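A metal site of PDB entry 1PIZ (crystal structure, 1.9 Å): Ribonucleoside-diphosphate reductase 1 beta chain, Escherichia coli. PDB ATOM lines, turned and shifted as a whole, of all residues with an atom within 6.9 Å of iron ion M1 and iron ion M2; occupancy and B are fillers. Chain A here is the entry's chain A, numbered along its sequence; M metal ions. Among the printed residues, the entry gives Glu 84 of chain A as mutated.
The backbone carbonyl oxygen (O) of Trp 111 sits at hydrogen-bond distance from the side-chain hydroxyl (OG) of Ser 114, at 2.7 Å.
OE2 of Glu 204 sits at hydrogen-bond distance from NE2 of Gln 87, 2.7 Å away.
The side-chain carboxylate (OE2) of Glu 115 lies close to the indole nitrogen (NE1) of Trp 111, at 3.2 Å.
The side-chain carboxylate (OE2) of Glu 204 lies within hydrogen-bond range of the indole nitrogen (NE1) of Trp 111 (3.1 Å).
The backbone carbonyl oxygen (O) of Glu 84 lies close to the side-chain hydroxyl (OG) of Ser 119 (3.4 Å).
A ring nitrogen (NE2) of His 118 sits close to the backbone carbonyl oxygen (O) of Ser 114 (3.4 Å).
The backbone carbonyl oxygen (O) of Asp 237 lies close to a ring nitrogen (NE2) of His 241, at 3.5 Å.
OG of Ser 119 lies within hydrogen-bond range of O of Glu 115 (3.4 Å).
NE1 of Trp 111 touches iron ion M1, 3.6 Å away.
Phe 208 touches iron ion M1.
Within 4 Å of iron ion M1: Trp 111, Glu 115, Glu 204, Phe 208, Glu 238 and His 241.
The nearest printed residue that does not touch iron ion M1 is His 118 (5.1 Å).
Residues that only touch iron ion M2: Phe 208 (3.8 Å).
Within 4 Å of iron ion M2: Glu 84, Glu 115, His 118, Phe 208 and Glu 238.
The nearest printed residue that does not touch iron ion M2 is Ile 234 (4.2 Å).
Iron ion M1 is bound by the side-chain carboxylate of Glu 238 (1.9 Å), the side-chain carboxylate of Glu 204 (2.0 Å), the side-chain carboxylate of Glu 115 (2.0 Å) and a ring nitrogen (ND1) of His 241 (2.1 Å).
Iron ion M2 is bound by OE2 of Glu 238 (2.0 Å), ND1 of His 118 (2.1 Å), OE1 of Glu 115 (2.1 Å), OE1 of Glu 84 (2.2 Å) and OE2 of Glu 84 (2.3 Å).
Iron ion M2 has five donor atoms within binding distance.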
ATOM      1  N   GLN A  80       6.321 -23.260  28.033  1.00  0.00           N
ATOM      2  CA  GLN A  80       5.009 -23.676  27.539  1.00  0.00           C
ATOM      3  C   GLN A  80       4.813 -25.164  27.831  1.00  0.00           C
ATOM      4  O   GLN A  80       3.749 -25.588  28.304  1.00  0.00           O
ATOM      5  CB  GLN A  80       4.907 -23.414  26.026  1.00  0.00           C
ATOM      6  CG  GLN A  80       5.054 -21.949  25.601  1.00  0.00           C
ATOM      7  CD  GLN A  80       5.066 -21.756  24.076  1.00  0.00           C
ATOM      8  OE1 GLN A  80       5.776 -22.463  23.355  1.00  0.00           O
ATOM      9  NE2 GLN A  80       4.298 -20.774  23.601  1.00  0.00           N
ATOM     10  N   LEU A  83       3.967 -25.710  31.473  1.00  0.00           N
ATOM     11  CA  LEU A  83       2.572 -25.367  31.761  1.00  0.00           C
ATOM     12  C   LEU A  83       1.566 -26.380  31.230  1.00  0.00           C
ATOM     13  O   LEU A  83       0.572 -26.662  31.888  1.00  0.00           O
ATOM     14  CB  LEU A  83       2.242 -23.976  31.195  1.00  0.00           C
ATOM     15  CG  LEU A  83       2.944 -22.773  31.830  1.00  0.00           C
ATOM     16  CD1 LEU A  83       2.350 -21.493  31.236  1.00  0.00           C
ATOM     17  CD2 LEU A  83       2.754 -22.789  33.345  1.00  0.00           C
ATOM     18  N   GLU A  84       1.812 -26.921  30.041  1.00  0.00           N
ATOM     19  CA  GLU A  84       0.886 -27.904  29.477  1.00  0.00           C
ATOM     20  C   GLU A  84       0.979 -29.215  30.259  1.00  0.00           C
ATOM     21  O   GLU A  84      -0.028 -29.892  30.455  1.00  0.00           O
ATOM     22  CB  GLU A  84       1.205 -28.151  28.003  1.00  0.00           C
ATOM     23  CG  GLU A  84       1.095 -26.898  27.153  1.00  0.00           C
ATOM     24  CD  GLU A  84      -0.342 -26.426  26.951  1.00  0.00           C
ATOM     25  OE1 GLU A  84      -1.239 -26.915  27.653  1.00  0.00           O
ATOM     26  OE2 GLU A  84      -0.550 -25.554  26.098  1.00  0.00           O
ATOM     27  N   GLN A  87      -1.078 -28.519  33.261  1.00  0.00           N
ATOM     28  CA  GLN A  87      -2.493 -28.360  32.914  1.00  0.00           C
ATOM     29  C   GLN A  87      -3.146 -29.614  32.342  1.00  0.00           C
ATOM     30  O   GLN A  87      -4.371 -29.708  32.287  1.00  0.00           O
ATOM     31  CB  GLN A  87      -2.667 -27.186  31.943  1.00  0.00           C
ATOM     32  CG  GLN A  87      -2.548 -25.798  32.595  1.00  0.00           C
ATOM     33  CD  GLN A  87      -3.382 -25.663  33.853  1.00  0.00           C
ATOM     34  OE1 GLN A  87      -2.970 -26.086  34.938  1.00  0.00           O
ATOM     35  NE2 GLN A  87      -4.575 -25.100  33.722  1.00  0.00           N
ATOM     36  N   TRP A 111     -11.293 -30.197  28.838  1.00  0.00           N
ATOM     37  CA  TRP A 111     -10.290 -29.133  28.933  1.00  0.00           C
ATOM     38  C   TRP A 111      -8.915 -29.763  29.194  1.00  0.00           C
ATOM     39  O   TRP A 111      -7.943 -29.487  28.482  1.00  0.00           O
ATOM     40  CB  TRP A 111     -10.734 -28.172  30.051  1.00  0.00           C
ATOM     41  CG  TRP A 111      -9.713 -27.238  30.631  1.00  0.00           C
ATOM     42  CD1 TRP A 111      -8.532 -26.836  30.076  1.00  0.00           C
ATOM     43  CD2 TRP A 111      -9.840 -26.548  31.878  1.00  0.00           C
ATOM     44  NE1 TRP A 111      -7.904 -25.930  30.915  1.00  0.00           N
ATOM     45  CE2 TRP A 111      -8.688 -25.734  32.025  1.00  0.00           C
ATOM     46  CE3 TRP A 111     -10.809 -26.545  32.895  1.00  0.00           C
ATOM     47  CZ2 TRP A 111      -8.490 -24.920  33.149  1.00  0.00           C
ATOM     48  CZ3 TRP A 111     -10.613 -25.727  34.010  1.00  0.00           C
ATOM     49  CH2 TRP A 111      -9.455 -24.926  34.127  1.00  0.00           C
ATOM     50  N   SER A 114      -7.546 -31.666  26.160  1.00  0.00           N
ATOM     51  CA  SER A 114      -7.006 -30.793  25.120  1.00  0.00           C
ATOM     52  C   SER A 114      -5.608 -30.320  25.500  1.00  0.00           C
ATOM     53  O   SER A 114      -4.774 -30.083  24.628  1.00  0.00           O
ATOM     54  CB  SER A 114      -7.934 -29.596  24.878  1.00  0.00           C
ATOM     55  OG  SER A 114      -7.880 -28.678  25.947  1.00  0.00           O
ATOM     56  N   GLU A 115      -5.339 -30.178  26.798  1.00  0.00           N
ATOM     57  CA  GLU A 115      -4.025 -29.741  27.232  1.00  0.00           C
ATOM     58  C   GLU A 115      -3.002 -30.849  26.935  1.00  0.00           C
ATOM     59  O   GLU A 115      -1.844 -30.550  26.591  1.00  0.00           O
ATOM     60  CB  GLU A 115      -4.029 -29.401  28.734  1.00  0.00           C
ATOM     61  CG  GLU A 115      -5.086 -28.355  29.138  1.00  0.00           C
ATOM     62  CD  GLU A 115      -4.779 -26.942  28.673  1.00  0.00           C
ATOM     63  OE1 GLU A 115      -4.250 -26.771  27.541  1.00  0.00           O
ATOM     64  OE2 GLU A 115      -5.083 -25.988  29.410  1.00  0.00           O
ATOM     65  N   THR A 116      -3.400 -32.112  27.051  1.00  0.00           N
ATOM     66  CA  THR A 116      -2.465 -33.211  26.751  1.00  0.00           C
ATOM     67  C   THR A 116      -2.150 -33.226  25.263  1.00  0.00           C
ATOM     68  O   THR A 116      -1.057 -33.633  24.854  1.00  0.00           O
ATOM     69  CB  THR A 116      -3.015 -34.603  27.176  1.00  0.00           C
ATOM     70  OG1 THR A 116      -4.177 -34.942  26.395  1.00  0.00           O
ATOM     71  CG2 THR A 116      -3.351 -34.608  28.649  1.00  0.00           C
ATOM     72  N   HIS A 118      -1.873 -30.536  23.565  1.00  0.00           N
ATOM     73  CA  HIS A 118      -0.890 -29.462  23.441  1.00  0.00           C
ATOM     74  C   HIS A 118       0.486 -29.990  23.818  1.00  0.00           C
ATOM     75  O   HIS A 118       1.488 -29.678  23.161  1.00  0.00           O
ATOM     76  CB  HIS A 118      -1.285 -28.289  24.334  1.00  0.00           C
ATOM     77  CG  HIS A 118      -2.603 -27.664  23.973  1.00  0.00           C
ATOM     78  ND1 HIS A 118      -3.188 -26.691  24.738  1.00  0.00           N
ATOM     79  CD2 HIS A 118      -3.442 -27.896  22.936  1.00  0.00           C
ATOM     80  CE1 HIS A 118      -4.340 -26.345  24.191  1.00  0.00           C
ATOM     81  NE2 HIS A 118      -4.520 -27.065  23.095  1.00  0.00           N
ATOM     82  N   SER A 119       0.554 -30.780  24.881  1.00  0.00           N
ATOM     83  CA  SER A 119       1.835 -31.351  25.314  1.00  0.00           C
ATOM     84  C   SER A 119       2.405 -32.219  24.190  1.00  0.00           C
ATOM     85  O   SER A 119       3.604 -32.210  23.925  1.00  0.00           O
ATOM     86  CB  SER A 119       1.643 -32.232  26.564  1.00  0.00           C
ATOM     87  OG  SER A 119       1.262 -31.450  27.681  1.00  0.00           O
ATOM     88  N   TYR A 122       4.045 -30.205  21.501  1.00  0.00           N
ATOM     89  CA  TYR A 122       5.382 -29.713  21.828  1.00  0.00           C
ATOM     90  C   TYR A 122       6.450 -30.793  21.657  1.00  0.00           C
ATOM     91  O   TYR A 122       7.585 -30.498  21.284  1.00  0.00           O
ATOM     92  CB  TYR A 122       5.390 -29.132  23.245  1.00  0.00           C
ATOM     93  CG  TYR A 122       4.735 -27.769  23.297  1.00  0.00           C
ATOM     94  CD1 TYR A 122       5.234 -26.730  22.512  1.00  0.00           C
ATOM     95  CD2 TYR A 122       3.626 -27.524  24.094  1.00  0.00           C
ATOM     96  CE1 TYR A 122       4.645 -25.466  22.530  1.00  0.00           C
ATOM     97  CE2 TYR A 122       3.015 -26.253  24.111  1.00  0.00           C
ATOM     98  CZ  TYR A 122       3.542 -25.232  23.320  1.00  0.00           C
ATOM     99  OH  TYR A 122       2.967 -23.981  23.328  1.00  0.00           O
ATOM    100  N   GLU A 204      -4.105 -19.546  32.441  1.00  0.00           N
ATOM    101  CA  GLU A 204      -4.718 -19.717  31.121  1.00  0.00           C
ATOM    102  C   GLU A 204      -4.789 -18.419  30.291  1.00  0.00           C
ATOM    103  O   GLU A 204      -4.533 -18.430  29.089  1.00  0.00           O
ATOM    104  CB  GLU A 204      -6.147 -20.251  31.263  1.00  0.00           C
ATOM    105  CG  GLU A 204      -6.317 -21.636  31.918  1.00  0.00           C
ATOM    106  CD  GLU A 204      -5.937 -22.799  31.011  1.00  0.00           C
ATOM    107  OE1 GLU A 204      -5.957 -22.634  29.772  1.00  0.00           O
ATOM    108  OE2 GLU A 204      -5.612 -23.889  31.527  1.00  0.00           O
ATOM    109  N   PHE A 208      -0.002 -18.083  29.331  1.00  0.00           N
ATOM    110  CA  PHE A 208       0.029 -18.685  27.995  1.00  0.00           C
ATOM    111  C   PHE A 208       0.151 -17.634  26.895  1.00  0.00           C
ATOM    112  O   PHE A 208       0.877 -17.835  25.915  1.00  0.00           O
ATOM    113  CB  PHE A 208      -1.219 -19.535  27.734  1.00  0.00           C
ATOM    114  CG  PHE A 208      -1.139 -20.949  28.263  1.00  0.00           C
ATOM    115  CD1 PHE A 208      -0.019 -21.731  28.022  1.00  0.00           C
ATOM    116  CD2 PHE A 208      -2.212 -21.501  28.966  1.00  0.00           C
ATOM    117  CE1 PHE A 208       0.035 -23.061  28.473  1.00  0.00           C
ATOM    118  CE2 PHE A 208      -2.167 -22.816  29.414  1.00  0.00           C
ATOM    119  CZ  PHE A 208      -1.038 -23.600  29.171  1.00  0.00           C
ATOM    120  N   PHE A 212       2.776 -16.853  23.768  1.00  0.00           N
ATOM    121  CA  PHE A 212       2.362 -16.863  22.372  1.00  0.00           C
ATOM    122  C   PHE A 212       3.031 -15.706  21.624  1.00  0.00           C
ATOM    123  O   PHE A 212       3.449 -15.864  20.485  1.00  0.00           O
ATOM    124  CB  PHE A 212       0.839 -16.717  22.224  1.00  0.00           C
ATOM    125  CG  PHE A 212       0.057 -17.859  22.795  1.00  0.00           C
ATOM    126  CD1 PHE A 212       0.633 -19.120  22.932  1.00  0.00           C
ATOM    127  CD2 PHE A 212      -1.268 -17.687  23.175  1.00  0.00           C
ATOM    128  CE1 PHE A 212      -0.100 -20.179  23.447  1.00  0.00           C
ATOM    129  CE2 PHE A 212      -2.008 -18.735  23.697  1.00  0.00           C
ATOM    130  CZ  PHE A 212      -1.419 -19.989  23.834  1.00  0.00           C
ATOM    131  N   ILE A 234      -3.273 -24.023  19.398  1.00  0.00           N
ATOM    132  CA  ILE A 234      -3.259 -24.053  20.853  1.00  0.00           C
ATOM    133  C   ILE A 234      -3.982 -22.842  21.407  1.00  0.00           C
ATOM    134  O   ILE A 234      -4.829 -22.957  22.295  1.00  0.00           O
ATOM    135  CB  ILE A 234      -1.814 -24.072  21.397  1.00  0.00           C
ATOM    136  CG1 ILE A 234      -1.168 -25.421  21.101  1.00  0.00           C
ATOM    137  CG2 ILE A 234      -1.811 -23.801  22.897  1.00  0.00           C
ATOM    138  CD1 ILE A 234       0.251 -25.548  21.658  1.00  0.00           C
ATOM    139  N   ASP A 237      -7.641 -23.022  21.503  1.00  0.00           N
ATOM    140  CA  ASP A 237      -8.139 -23.836  22.615  1.00  0.00           C
ATOM    141  C   ASP A 237      -8.067 -23.048  23.928  1.00  0.00           C
ATOM    142  O   ASP A 237      -9.001 -23.076  24.723  1.00  0.00           O
ATOM    143  CB  ASP A 237      -7.332 -25.142  22.750  1.00  0.00           C
ATOM    144  CG  ASP A 237      -7.528 -26.088  21.586  1.00  0.00           C
ATOM    145  OD1 ASP A 237      -8.589 -26.019  20.912  1.00  0.00           O
ATOM    146  OD2 ASP A 237      -6.627 -26.930  21.350  1.00  0.00           O
ATOM    147  N   GLU A 238      -6.950 -22.353  24.155  1.00  0.00           N
ATOM    148  CA  GLU A 238      -6.786 -21.588  25.382  1.00  0.00           C
ATOM    149  C   GLU A 238      -7.890 -20.531  25.530  1.00  0.00           C
ATOM    150  O   GLU A 238      -8.291 -20.204  26.653  1.00  0.00           O
ATOM    151  CB  GLU A 238      -5.411 -20.908  25.441  1.00  0.00           C
ATOM    152  CG  GLU A 238      -4.192 -21.837  25.353  1.00  0.00           C
ATOM    153  CD  GLU A 238      -4.223 -23.010  26.332  1.00  0.00           C
ATOM    154  OE1 GLU A 238      -5.003 -22.968  27.309  1.00  0.00           O
ATOM    155  OE2 GLU A 238      -3.453 -23.974  26.125  1.00  0.00           O
ATOM    156  N   ALA A 239      -8.362 -20.005  24.409  1.00  0.00           N
ATOM    157  CA  ALA A 239      -9.421 -19.002  24.448  1.00  0.00           C
ATOM    158  C   ALA A 239     -10.692 -19.599  25.065  1.00  0.00           C
ATOM    159  O   ALA A 239     -11.409 -18.933  25.815  1.00  0.00           O
ATOM    160  CB  ALA A 239      -9.714 -18.477  23.040  1.00  0.00           C
ATOM    161  N   HIS A 241     -10.683 -22.226  27.141  1.00  0.00           N
ATOM    162  CA  HIS A 241     -10.313 -22.520  28.521  1.00  0.00           C
ATOM    163  C   HIS A 241     -10.478 -21.305  29.421  1.00  0.00           C
ATOM    164  O   HIS A 241     -11.082 -21.393  30.489  1.00  0.00           O
ATOM    165  CB  HIS A 241      -8.873 -23.033  28.587  1.00  0.00           C
ATOM    166  CG  HIS A 241      -8.623 -24.262  27.769  1.00  0.00           C
ATOM    167  ND1 HIS A 241      -7.365 -24.812  27.621  1.00  0.00           N
ATOM    168  CD2 HIS A 241      -9.463 -25.051  27.053  1.00  0.00           C
ATOM    169  CE1 HIS A 241      -7.442 -25.873  26.835  1.00  0.00           C
ATOM    170  NE2 HIS A 241      -8.705 -26.042  26.479  1.00  0.00           N
ATOM    171  N   LEU A 242      -9.930 -20.162  29.004  1.00  0.00           N
ATOM    172  CA  LEU A 242     -10.057 -18.973  29.845  1.00  0.00           C
ATOM    173  C   LEU A 242     -11.512 -18.499  29.869  1.00  0.00           C
ATOM    174  O   LEU A 242     -11.951 -17.906  30.854  1.00  0.00           O
ATOM    175  CB  LEU A 242      -9.107 -17.877  29.361  1.00  0.00           C
ATOM    176  CG  LEU A 242      -9.347 -17.100  28.069  1.00  0.00           C
ATOM    177  CD1 LEU A 242     -10.376 -15.997  28.297  1.00  0.00           C
ATOM    178  CD2 LEU A 242      -8.023 -16.473  27.624  1.00  0.00           C
HETATM  179 FE    FE M   1      -5.650 -24.231  28.621  1.00  0.00          FE
HETATM  180 FE    FE M   2      -2.755 -25.753  26.517  1.00  0.00          FE
